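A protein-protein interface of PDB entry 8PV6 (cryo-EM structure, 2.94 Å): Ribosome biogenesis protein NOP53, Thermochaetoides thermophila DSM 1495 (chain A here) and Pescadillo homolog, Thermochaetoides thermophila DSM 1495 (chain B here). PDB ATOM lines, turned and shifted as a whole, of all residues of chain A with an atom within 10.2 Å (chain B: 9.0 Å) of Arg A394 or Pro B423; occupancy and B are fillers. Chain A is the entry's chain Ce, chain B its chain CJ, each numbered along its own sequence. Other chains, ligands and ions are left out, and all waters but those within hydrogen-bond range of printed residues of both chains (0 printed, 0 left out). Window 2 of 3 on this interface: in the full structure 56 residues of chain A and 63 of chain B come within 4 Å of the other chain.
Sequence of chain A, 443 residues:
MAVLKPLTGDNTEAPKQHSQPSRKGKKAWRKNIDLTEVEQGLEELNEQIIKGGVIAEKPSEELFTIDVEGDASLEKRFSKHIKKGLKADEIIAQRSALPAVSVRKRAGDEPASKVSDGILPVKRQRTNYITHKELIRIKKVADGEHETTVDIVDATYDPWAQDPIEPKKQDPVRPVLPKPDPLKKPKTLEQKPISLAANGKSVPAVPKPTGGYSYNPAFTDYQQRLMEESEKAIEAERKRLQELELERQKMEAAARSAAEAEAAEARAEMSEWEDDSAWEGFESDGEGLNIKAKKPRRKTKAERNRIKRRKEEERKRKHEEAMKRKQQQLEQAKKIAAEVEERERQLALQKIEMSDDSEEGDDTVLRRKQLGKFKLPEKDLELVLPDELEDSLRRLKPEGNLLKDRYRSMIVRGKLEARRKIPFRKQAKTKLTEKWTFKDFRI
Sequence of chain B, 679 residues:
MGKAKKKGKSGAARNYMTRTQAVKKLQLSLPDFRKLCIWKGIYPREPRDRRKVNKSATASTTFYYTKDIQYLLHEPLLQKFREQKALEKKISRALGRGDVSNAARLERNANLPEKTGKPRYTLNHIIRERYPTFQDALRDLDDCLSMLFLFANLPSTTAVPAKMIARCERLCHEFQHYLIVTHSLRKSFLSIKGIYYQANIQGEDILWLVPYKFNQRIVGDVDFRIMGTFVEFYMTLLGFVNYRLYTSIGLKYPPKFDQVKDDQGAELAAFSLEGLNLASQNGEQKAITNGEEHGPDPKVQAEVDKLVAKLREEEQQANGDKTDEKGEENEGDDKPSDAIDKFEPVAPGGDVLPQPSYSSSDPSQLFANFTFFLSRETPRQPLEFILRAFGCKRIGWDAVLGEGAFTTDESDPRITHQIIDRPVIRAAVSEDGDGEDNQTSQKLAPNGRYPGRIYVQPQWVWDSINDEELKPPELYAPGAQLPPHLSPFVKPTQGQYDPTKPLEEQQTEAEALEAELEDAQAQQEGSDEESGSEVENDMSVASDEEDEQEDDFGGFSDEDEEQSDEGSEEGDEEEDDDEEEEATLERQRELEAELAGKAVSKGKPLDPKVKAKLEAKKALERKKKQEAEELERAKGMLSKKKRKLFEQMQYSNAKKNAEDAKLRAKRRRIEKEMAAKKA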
ATOM      1  N   TYR A 215     -23.895 -20.032 -16.008  1.00  0.00           N
ATOM      2  CA  TYR A 215     -23.293 -20.190 -14.689  1.00  0.00           C
ATOM      3  C   TYR A 215     -24.135 -21.096 -13.800  1.00  0.00           C
ATOM      4  O   TYR A 215     -23.603 -21.728 -12.880  1.00  0.00           O
ATOM      5  CB  TYR A 215     -23.092 -18.824 -14.038  1.00  0.00           C
ATOM      6  CG  TYR A 215     -24.288 -18.305 -13.278  1.00  0.00           C
ATOM      7  CD1 TYR A 215     -25.416 -17.849 -13.946  1.00  0.00           C
ATOM      8  CD2 TYR A 215     -24.282 -18.260 -11.891  1.00  0.00           C
ATOM      9  CE1 TYR A 215     -26.510 -17.371 -13.250  1.00  0.00           C
ATOM     10  CE2 TYR A 215     -25.368 -17.786 -11.189  1.00  0.00           C
ATOM     11  CZ  TYR A 215     -26.478 -17.343 -11.872  1.00  0.00           C
ATOM     12  OH  TYR A 215     -27.560 -16.869 -11.173  1.00  0.00           O
ATOM     13  N   GLU A 390     -21.414 -24.235  -7.706  1.00  0.00           N
ATOM     14  CA  GLU A 390     -21.870 -23.353  -6.646  1.00  0.00           C
ATOM     15  C   GLU A 390     -23.335 -23.003  -6.870  1.00  0.00           C
ATOM     16  O   GLU A 390     -23.932 -23.340  -7.895  1.00  0.00           O
ATOM     17  CB  GLU A 390     -21.009 -22.087  -6.591  1.00  0.00           C
ATOM     18  CG  GLU A 390     -19.534 -22.363  -6.346  1.00  0.00           C
ATOM     19  CD  GLU A 390     -19.229 -22.708  -4.902  1.00  0.00           C
ATOM     20  OE1 GLU A 390     -20.071 -22.416  -4.025  1.00  0.00           O
ATOM     21  OE2 GLU A 390     -18.145 -23.270  -4.642  1.00  0.00           O
ATOM     22  N   ASP A 391     -23.917 -22.314  -5.890  1.00  0.00           N
ATOM     23  CA  ASP A 391     -25.338 -21.991  -5.916  1.00  0.00           C
ATOM     24  C   ASP A 391     -25.613 -20.494  -5.849  1.00  0.00           C
ATOM     25  O   ASP A 391     -26.746 -20.098  -5.550  1.00  0.00           O
ATOM     26  CB  ASP A 391     -26.060 -22.705  -4.771  1.00  0.00           C
ATOM     27  CG  ASP A 391     -25.335 -22.563  -3.448  1.00  0.00           C
ATOM     28  OD1 ASP A 391     -24.241 -21.962  -3.428  1.00  0.00           O
ATOM     29  OD2 ASP A 391     -25.858 -23.056  -2.426  1.00  0.00           O
ATOM     30  N   SER A 392     -24.618 -19.650  -6.116  1.00  0.00           N
ATOM     31  CA  SER A 392     -24.803 -18.209  -6.035  1.00  0.00           C
ATOM     32  C   SER A 392     -23.926 -17.513  -7.063  1.00  0.00           C
ATOM     33  O   SER A 392     -22.939 -18.074  -7.547  1.00  0.00           O
ATOM     34  CB  SER A 392     -24.480 -17.679  -4.632  1.00  0.00           C
ATOM     35  OG  SER A 392     -23.125 -17.920  -4.298  1.00  0.00           O
ATOM     36  N   LEU A 393     -24.305 -16.276  -7.394  1.00  0.00           N
ATOM     37  CA  LEU A 393     -23.519 -15.479  -8.330  1.00  0.00           C
ATOM     38  C   LEU A 393     -22.227 -14.990  -7.689  1.00  0.00           C
ATOM     39  O   LEU A 393     -21.215 -14.813  -8.378  1.00  0.00           O
ATOM     40  CB  LEU A 393     -24.356 -14.301  -8.834  1.00  0.00           C
ATOM     41  CG  LEU A 393     -23.736 -13.345  -9.856  1.00  0.00           C
ATOM     42  CD1 LEU A 393     -23.344 -14.091 -11.112  1.00  0.00           C
ATOM     43  CD2 LEU A 393     -24.693 -12.216 -10.186  1.00  0.00           C
ATOM     44  N   ARG A 394     -22.245 -14.761  -6.373  1.00  0.00           N
ATOM     45  CA  ARG A 394     -21.059 -14.261  -5.683  1.00  0.00           C
ATOM     46  C   ARG A 394     -19.946 -15.303  -5.668  1.00  0.00           C
ATOM     47  O   ARG A 394     -18.767 -14.966  -5.826  1.00  0.00           O
ATOM     48  CB  ARG A 394     -21.429 -13.836  -4.261  1.00  0.00           C
ATOM     49  CG  ARG A 394     -20.249 -13.489  -3.372  1.00  0.00           C
ATOM     50  CD  ARG A 394     -20.693 -13.227  -1.943  1.00  0.00           C
ATOM     51  NE  ARG A 394     -21.614 -14.249  -1.459  1.00  0.00           N
ATOM     52  CZ  ARG A 394     -21.252 -15.458  -1.053  1.00  0.00           C
ATOM     53  NH1 ARG A 394     -19.983 -15.831  -1.034  1.00  0.00           N
ATOM     54  NH2 ARG A 394     -22.187 -16.314  -0.652  1.00  0.00           N
ATOM     55  N   ARG A 395     -20.300 -16.575  -5.505  1.00  0.00           N
ATOM     56  CA  ARG A 395     -19.325 -17.656  -5.459  1.00  0.00           C
ATOM     57  C   ARG A 395     -18.947 -18.182  -6.838  1.00  0.00           C
ATOM     58  O   ARG A 395     -18.477 -19.318  -6.939  1.00  0.00           O
ATOM     59  CB  ARG A 395     -19.857 -18.813  -4.608  1.00  0.00           C
ATOM     60  CG  ARG A 395     -20.064 -18.469  -3.146  1.00  0.00           C
ATOM     61  CD  ARG A 395     -19.608 -19.597  -2.240  1.00  0.00           C
ATOM     62  NE  ARG A 395     -18.171 -19.820  -2.345  1.00  0.00           N
ATOM     63  CZ  ARG A 395     -17.577 -20.993  -2.167  1.00  0.00           C
ATOM     64  NH1 ARG A 395     -18.269 -22.078  -1.863  1.00  0.00           N
ATOM     65  NH2 ARG A 395     -16.256 -21.076  -2.292  1.00  0.00           N
ATOM     66  N   LEU A 396     -19.147 -17.393  -7.892  1.00  0.00           N
ATOM     67  CA  LEU A 396     -18.860 -17.854  -9.244  1.00  0.00           C
ATOM     68  C   LEU A 396     -17.361 -18.015  -9.455  1.00  0.00           C
ATOM     69  O   LEU A 396     -16.550 -17.278  -8.889  1.00  0.00           O
ATOM     70  CB  LEU A 396     -19.439 -16.870 -10.265  1.00  0.00           C
ATOM     71  CG  LEU A 396     -19.671 -17.302 -11.717  1.00  0.00           C
ATOM     72  CD1 LEU A 396     -20.844 -16.538 -12.274  1.00  0.00           C
ATOM     73  CD2 LEU A 396     -18.462 -17.048 -12.594  1.00  0.00           C
ATOM     74  N   LYS A 397     -16.997 -18.999 -10.278  1.00  0.00           N
ATOM     75  CA  LYS A 397     -15.618 -19.245 -10.686  1.00  0.00           C
ATOM     76  C   LYS A 397     -15.510 -18.913 -12.168  1.00  0.00           C
ATOM     77  O   LYS A 397     -15.884 -19.733 -13.019  1.00  0.00           O
ATOM     78  CB  LYS A 397     -15.225 -20.701 -10.426  1.00  0.00           C
ATOM     79  CG  LYS A 397     -13.746 -20.995 -10.598  1.00  0.00           C
ATOM     80  CD  LYS A 397     -12.928 -20.342  -9.505  1.00  0.00           C
ATOM     81  CE  LYS A 397     -13.304 -20.899  -8.141  1.00  0.00           C
ATOM     82  NZ  LYS A 397     -12.916 -22.328  -7.997  1.00  0.00           N
ATOM     83  N   PRO A 398     -15.045 -17.716 -12.529  1.00  0.00           N
ATOM     84  CA  PRO A 398     -14.919 -17.370 -13.950  1.00  0.00           C
ATOM     85  C   PRO A 398     -13.871 -18.230 -14.640  1.00  0.00           C
ATOM     86  O   PRO A 398     -12.769 -18.433 -14.127  1.00  0.00           O
ATOM     87  CB  PRO A 398     -14.511 -15.892 -13.927  1.00  0.00           C
ATOM     88  CG  PRO A 398     -14.100 -15.601 -12.529  1.00  0.00           C
ATOM     89  CD  PRO A 398     -14.816 -16.561 -11.648  1.00  0.00           C
ATOM     90  N   LEU B 190     -25.787 -14.506 -18.203  1.00  0.00           N
ATOM     91  CA  LEU B 190     -24.684 -14.711 -17.264  1.00  0.00           C
ATOM     92  C   LEU B 190     -24.057 -16.070 -17.543  1.00  0.00           C
ATOM     93  O   LEU B 190     -24.612 -17.106 -17.170  1.00  0.00           O
ATOM     94  CB  LEU B 190     -25.171 -14.623 -15.823  1.00  0.00           C
ATOM     95  CG  LEU B 190     -25.680 -13.283 -15.310  1.00  0.00           C
ATOM     96  CD1 LEU B 190     -26.517 -13.493 -14.067  1.00  0.00           C
ATOM     97  CD2 LEU B 190     -24.506 -12.373 -15.016  1.00  0.00           C
ATOM     98  N   TYR B 212     -16.516 -10.160 -15.991  1.00  0.00           N
ATOM     99  CA  TYR B 212     -16.893  -9.907 -14.608  1.00  0.00           C
ATOM    100  C   TYR B 212     -15.879  -8.977 -13.954  1.00  0.00           C
ATOM    101  O   TYR B 212     -14.689  -8.994 -14.279  1.00  0.00           O
ATOM    102  CB  TYR B 212     -16.979 -11.218 -13.829  1.00  0.00           C
ATOM    103  CG  TYR B 212     -18.223 -12.029 -14.098  1.00  0.00           C
ATOM    104  CD1 TYR B 212     -19.476 -11.553 -13.741  1.00  0.00           C
ATOM    105  CD2 TYR B 212     -18.144 -13.278 -14.698  1.00  0.00           C
ATOM    106  CE1 TYR B 212     -20.615 -12.292 -13.980  1.00  0.00           C
ATOM    107  CE2 TYR B 212     -19.276 -14.025 -14.940  1.00  0.00           C
ATOM    108  CZ  TYR B 212     -20.508 -13.528 -14.580  1.00  0.00           C
ATOM    109  OH  TYR B 212     -21.641 -14.270 -14.820  1.00  0.00           O
ATOM    110  N   PHE B 214     -13.429  -8.219 -11.894  1.00  0.00           N
ATOM    111  CA  PHE B 214     -12.416  -8.839 -11.051  1.00  0.00           C
ATOM    112  C   PHE B 214     -11.049  -8.400 -11.552  1.00  0.00           C
ATOM    113  O   PHE B 214     -10.927  -7.475 -12.358  1.00  0.00           O
ATOM    114  CB  PHE B 214     -12.524 -10.369 -11.059  1.00  0.00           C
ATOM    115  CG  PHE B 214     -13.751 -10.900 -10.377  1.00  0.00           C
ATOM    116  CD1 PHE B 214     -13.934 -10.727  -9.017  1.00  0.00           C
ATOM    117  CD2 PHE B 214     -14.710 -11.593 -11.093  1.00  0.00           C
ATOM    118  CE1 PHE B 214     -15.059 -11.220  -8.385  1.00  0.00           C
ATOM    119  CE2 PHE B 214     -15.839 -12.090 -10.469  1.00  0.00           C
ATOM    120  CZ  PHE B 214     -16.012 -11.903  -9.113  1.00  0.00           C
ATOM    121  N   ARG B 376     -24.205  -4.729  -1.179  1.00  0.00           N
ATOM    122  CA  ARG B 376     -22.772  -4.565  -1.387  1.00  0.00           C
ATOM    123  C   ARG B 376     -22.192  -5.686  -2.241  1.00  0.00           C
ATOM    124  O   ARG B 376     -21.288  -5.457  -3.053  1.00  0.00           O
ATOM    125  CB  ARG B 376     -22.069  -4.497  -0.031  1.00  0.00           C
ATOM    126  CG  ARG B 376     -20.586  -4.219  -0.096  1.00  0.00           C
ATOM    127  CD  ARG B 376     -20.081  -3.708   1.238  1.00  0.00           C
ATOM    128  NE  ARG B 376     -20.214  -4.698   2.300  1.00  0.00           N
ATOM    129  CZ  ARG B 376     -21.002  -4.559   3.357  1.00  0.00           C
ATOM    130  NH1 ARG B 376     -21.746  -3.479   3.529  1.00  0.00           N
ATOM    131  NH2 ARG B 376     -21.043  -5.529   4.267  1.00  0.00           N
ATOM    132  N   GLU B 377     -22.712  -6.899  -2.091  1.00  0.00           N
ATOM    133  CA  GLU B 377     -22.168  -8.071  -2.763  1.00  0.00           C
ATOM    134  C   GLU B 377     -22.718  -8.268  -4.172  1.00  0.00           C
ATOM    135  O   GLU B 377     -22.337  -9.236  -4.838  1.00  0.00           O
ATOM    136  CB  GLU B 377     -22.443  -9.322  -1.922  1.00  0.00           C
ATOM    137  CG  GLU B 377     -23.880  -9.816  -1.995  1.00  0.00           C
ATOM    138  CD  GLU B 377     -24.826  -9.050  -1.089  1.00  0.00           C
ATOM    139  OE1 GLU B 377     -24.357  -8.187  -0.319  1.00  0.00           O
ATOM    140  OE2 GLU B 377     -26.046  -9.314  -1.149  1.00  0.00           O
ATOM    141  N   THR B 378     -23.590  -7.381  -4.641  1.00  0.00           N
ATOM    142  CA  THR B 378     -24.239  -7.537  -5.933  1.00  0.00           C
ATOM    143  C   THR B 378     -23.481  -6.779  -7.022  1.00  0.00           C
ATOM    144  O   THR B 378     -22.894  -5.726  -6.757  1.00  0.00           O
ATOM    145  CB  THR B 378     -25.684  -7.031  -5.873  1.00  0.00           C
ATOM    146  OG1 THR B 378     -25.690  -5.620  -5.625  1.00  0.00           O
ATOM    147  CG2 THR B 378     -26.448  -7.735  -4.766  1.00  0.00           C
ATOM    148  N   PRO B 379     -23.466  -7.293  -8.263  1.00  0.00           N
ATOM    149  CA  PRO B 379     -22.732  -6.604  -9.336  1.00  0.00           C
ATOM    150  C   PRO B 379     -23.420  -5.330  -9.815  1.00  0.00           C
ATOM    151  O   PRO B 379     -24.395  -5.353 -10.587  1.00  0.00           O
ATOM    152  CB  PRO B 379     -22.652  -7.666 -10.438  1.00  0.00           C
ATOM    153  CG  PRO B 379     -23.793  -8.580 -10.172  1.00  0.00           C
ATOM    154  CD  PRO B 379     -23.945  -8.621  -8.686  1.00  0.00           C
ATOM    155  N   ILE B 420     -30.228  -9.502  -2.895  1.00  0.00           N
ATOM    156  CA  ILE B 420     -29.465 -10.150  -1.837  1.00  0.00           C
ATOM    157  C   ILE B 420     -28.754 -11.371  -2.404  1.00  0.00           C
ATOM    158  O   ILE B 420     -29.352 -12.213  -3.078  1.00  0.00           O
ATOM    159  CB  ILE B 420     -30.361 -10.562  -0.646  1.00  0.00           C
ATOM    160  CG1 ILE B 420     -31.077  -9.346  -0.063  1.00  0.00           C
ATOM    161  CG2 ILE B 420     -29.550 -11.261   0.436  1.00  0.00           C
ATOM    162  CD1 ILE B 420     -30.146  -8.337   0.561  1.00  0.00           C
ATOM    163  N   ASP B 421     -27.453 -11.461  -2.121  1.00  0.00           N
ATOM    164  CA  ASP B 421     -26.675 -12.632  -2.507  1.00  0.00           C
ATOM    165  C   ASP B 421     -25.759 -13.082  -1.374  1.00  0.00           C
ATOM    166  O   ASP B 421     -24.576 -13.359  -1.598  1.00  0.00           O
ATOM    167  CB  ASP B 421     -25.861 -12.344  -3.771  1.00  0.00           C
ATOM    168  CG  ASP B 421     -25.546 -13.599  -4.559  1.00  0.00           C
ATOM    169  OD1 ASP B 421     -25.933 -14.698  -4.109  1.00  0.00           O
ATOM    170  OD2 ASP B 421     -24.911 -13.488  -5.628  1.00  0.00           O
ATOM    171  N   ARG B 422     -26.290 -13.156  -0.159  1.00  0.00           N
ATOM    172  CA  ARG B 422     -25.569 -13.635   1.008  1.00  0.00           C
ATOM    173  C   ARG B 422     -26.267 -14.858   1.592  1.00  0.00           C
ATOM    174  O   ARG B 422     -27.495 -14.979   1.513  1.00  0.00           O
ATOM    175  CB  ARG B 422     -25.467 -12.544   2.085  1.00  0.00           C
ATOM    176  CG  ARG B 422     -24.855 -11.247   1.602  1.00  0.00           C
ATOM    177  CD  ARG B 422     -24.713 -10.250   2.740  1.00  0.00           C
ATOM    178  NE  ARG B 422     -23.501 -10.478   3.516  1.00  0.00           N
ATOM    179  CZ  ARG B 422     -22.325  -9.925   3.251  1.00  0.00           C
ATOM    180  NH1 ARG B 422     -22.165  -9.098   2.230  1.00  0.00           N
ATOM    181  NH2 ARG B 422     -21.284 -10.207   4.028  1.00  0.00           N
ATOM    182  N   PRO B 423     -25.509 -15.792   2.189  1.00  0.00           N
ATOM    183  CA  PRO B 423     -26.127 -16.965   2.817  1.00  0.00           C
ATOM    184  C   PRO B 423     -26.680 -16.666   4.207  1.00  0.00           C
ATOM    185  O   PRO B 423     -27.594 -15.851   4.327  1.00  0.00           O
ATOM    186  CB  PRO B 423     -24.970 -17.961   2.896  1.00  0.00           C
ATOM    187  CG  PRO B 423     -23.765 -17.103   3.033  1.00  0.00           C
ATOM    188  CD  PRO B 423     -24.036 -15.871   2.212  1.00  0.00           C
ATOM    189  N   ARG B 449     -35.438  -9.175   7.953  1.00  0.00           N
ATOM    190  CA  ARG B 449     -36.054  -8.723   6.711  1.00  0.00           C
ATOM    191  C   ARG B 449     -37.104  -7.670   7.040  1.00  0.00           C
ATOM    192  O   ARG B 449     -37.977  -7.902   7.882  1.00  0.00           O
ATOM    193  CB  ARG B 449     -36.686  -9.892   5.954  1.00  0.00           C
ATOM    194  CG  ARG B 449     -35.759 -11.079   5.738  1.00  0.00           C
ATOM    195  CD  ARG B 449     -34.466 -10.671   5.053  1.00  0.00           C
ATOM    196  NE  ARG B 449     -33.675 -11.830   4.654  1.00  0.00           N
ATOM    197  CZ  ARG B 449     -32.469 -11.764   4.107  1.00  0.00           C
ATOM    198  NH1 ARG B 449     -31.878 -10.603   3.877  1.00  0.00           N
ATOM    199  NH2 ARG B 449     -31.841 -12.890   3.785  1.00  0.00           N
ATOM    200  N   GLN B 457     -32.407 -12.690  -5.387  1.00  0.00           N
ATOM    201  CA  GLN B 457     -31.063 -12.901  -5.895  1.00  0.00           C
ATOM    202  C   GLN B 457     -30.922 -12.248  -7.265  1.00  0.00           C
ATOM    203  O   GLN B 457     -31.924 -11.995  -7.940  1.00  0.00           O
ATOM    204  CB  GLN B 457     -30.766 -14.401  -5.963  1.00  0.00           C
ATOM    205  CG  GLN B 457     -30.944 -15.109  -4.630  1.00  0.00           C
ATOM    206  CD  GLN B 457     -30.280 -16.471  -4.593  1.00  0.00           C
ATOM    207  OE1 GLN B 457     -29.285 -16.706  -5.276  1.00  0.00           O
ATOM    208  NE2 GLN B 457     -30.828 -17.376  -3.791  1.00  0.00           N
ATOM    209  N   PRO B 458     -29.691 -11.929  -7.700  1.00  0.00           N
ATOM    210  CA  PRO B 458     -29.529 -11.199  -8.974  1.00  0.00           C
ATOM    211  C   PRO B 458     -30.020 -11.927 -10.221  1.00  0.00           C
ATOM    212  O   PRO B 458     -30.247 -11.269 -11.243  1.00  0.00           O
ATOM    213  CB  PRO B 458     -28.015 -10.956  -9.041  1.00  0.00           C
ATOM    214  CG  PRO B 458     -27.567 -10.970  -7.643  1.00  0.00           C
ATOM    215  CD  PRO B 458     -28.427 -11.968  -6.940  1.00  0.00           C
ATOM    216  N   GLN B 459     -30.199 -13.252 -10.180  1.00  0.00           N
ATOM    217  CA  GLN B 459     -30.669 -13.969 -11.364  1.00  0.00           C
ATOM    218  C   GLN B 459     -32.115 -13.618 -11.701  1.00  0.00           C
ATOM    219  O   GLN B 459     -32.549 -13.803 -12.847  1.00  0.00           O
ATOM    220  CB  GLN B 459     -30.515 -15.479 -11.158  1.00  0.00           C
ATOM    221  CG  GLN B 459     -30.668 -16.313 -12.429  1.00  0.00           C
ATOM    222  CD  GLN B 459     -30.435 -17.792 -12.203  1.00  0.00           C
ATOM    223  OE1 GLN B 459     -29.498 -18.187 -11.513  1.00  0.00           O
ATOM    224  NE2 GLN B 459     -31.291 -18.620 -12.789  1.00  0.00           N
ATOM    225  N   PRO B 478     -33.606 -15.567  -1.031  1.00  0.00           N
ATOM    226  CA  PRO B 478     -32.262 -15.888  -0.532  1.00  0.00           C
ATOM    227  C   PRO B 478     -32.228 -17.231   0.185  1.00  0.00           C
ATOM    228  O   PRO B 478     -33.113 -17.556   0.979  1.00  0.00           O
ATOM    229  CB  PRO B 478     -31.958 -14.731   0.425  1.00  0.00           C
ATOM    230  CG  PRO B 478     -32.797 -13.611  -0.061  1.00  0.00           C
ATOM    231  CD  PRO B 478     -34.055 -14.239  -0.577  1.00  0.00           C
ATOM    232  N   GLY B 479     -31.189 -18.012  -0.102  1.00  0.00           N
ATOM    233  CA  GLY B 479     -31.031 -19.327   0.475  1.00  0.00           C
ATOM    234  C   GLY B 479     -31.734 -20.444  -0.265  1.00  0.00           C
ATOM    235  O   GLY B 479     -31.562 -21.613   0.103  1.00  0.00           O
ATOM    236  N   ALA B 480     -32.517 -20.128  -1.291  1.00  0.00           N
ATOM    237  CA  ALA B 480     -33.237 -21.147  -2.035  1.00  0.00           C
ATOM    238  C   ALA B 480     -32.476 -21.533  -3.300  1.00  0.00           C
ATOM    239  O   ALA B 480     -31.591 -20.813  -3.773  1.00  0.00           O
ATOM    240  CB  ALA B 480     -34.641 -20.660  -2.396  1.00  0.00           C
ATOM    241  N   LEU B 482     -31.959 -21.754  -7.027  1.00  0.00           N
ATOM    242  CA  LEU B 482     -32.420 -20.950  -8.144  1.00  0.00           C
ATOM    243  C   LEU B 482     -32.840 -21.840  -9.313  1.00  0.00           C
ATOM    244  O   LEU B 482     -32.304 -22.936  -9.495  1.00  0.00           O
ATOM    245  CB  LEU B 482     -31.325 -19.990  -8.593  1.00  0.00           C
ATOM    246  CG  LEU B 482     -30.969 -18.863  -7.623  1.00  0.00           C
ATOM    247  CD1 LEU B 482     -29.933 -17.949  -8.243  1.00  0.00           C
ATOM    248  CD2 LEU B 482     -32.213 -18.081  -7.238  1.00  0.00           C
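O of Leu B190 sits at hydrogen-bond distance from N of Tyr A215, 3.2 Å away. N of Leu A393 sits close to OD2 of Asp B421, at 3.4 Å. The backbone NH (N) of Arg A394 sits at hydrogen-bond distance from the side-chain carboxylate (OD2) of Asp B421 (3.0 Å). The side-chain hydroxyl (OH) of Tyr A215 lies close to the side-chain amide oxygen (OE1) of Gln B459.
OG of Ser A392 lies close to N of Arg A395, 3.4 Å away. The side-chain carboxylate (OE2) of Glu B377 lies within hydrogen-bond range of the backbone NH (N) of Asp B421.
Tyr A215 touches Leu B482 (OH to CD1, 3.9 Å). CB of Ser A392 touches OD1 of Asp B421, at 3.4 Å. Leu A393 touches Pro B379. CB of Pro B458 touches CD2 of Leu A393 (3.7 Å). Pro B423 touches Arg A394. Leu A396 touches Tyr B212.
Arg A394 touches just these residues of chain B: Asp B421 (3.0 Å) and Pro B423 (3.4 Å). Of the printed residues of chain A, Pro B423 touches Arg A394. Printed residues of chain B within 4 Å of Ser A392: Asp B421 (3.4 Å). Of the printed residues of chain B, Leu A396 touches Tyr B212. Printed residues of chain B within 4 Å of Tyr A215: Leu B190, Gln B459 and Leu B482. Of the printed residues of chain A, Gln B459 touches Tyr A215. Arg B449 touches none of the printed residues of chain A. The nearest residue of chain A that does not touch Pro B423 is Ser A392 (6.9 Å). The nearest printed residue of chain B that does not touch Leu A393 is Tyr B212 (4.1 Å).
Of the 10 printed residues of chain A, 5 touch a printed residue of chain B. Printed residues of chain A that touch a printed residue of chain B: Tyr A215, Ser A392, Leu A393, Arg A394 and Leu A396. Hydrophobic or aromatic side chains of chain A within 4 Å of the printed part of chain B: Tyr A215, Leu A393 and Leu A396.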
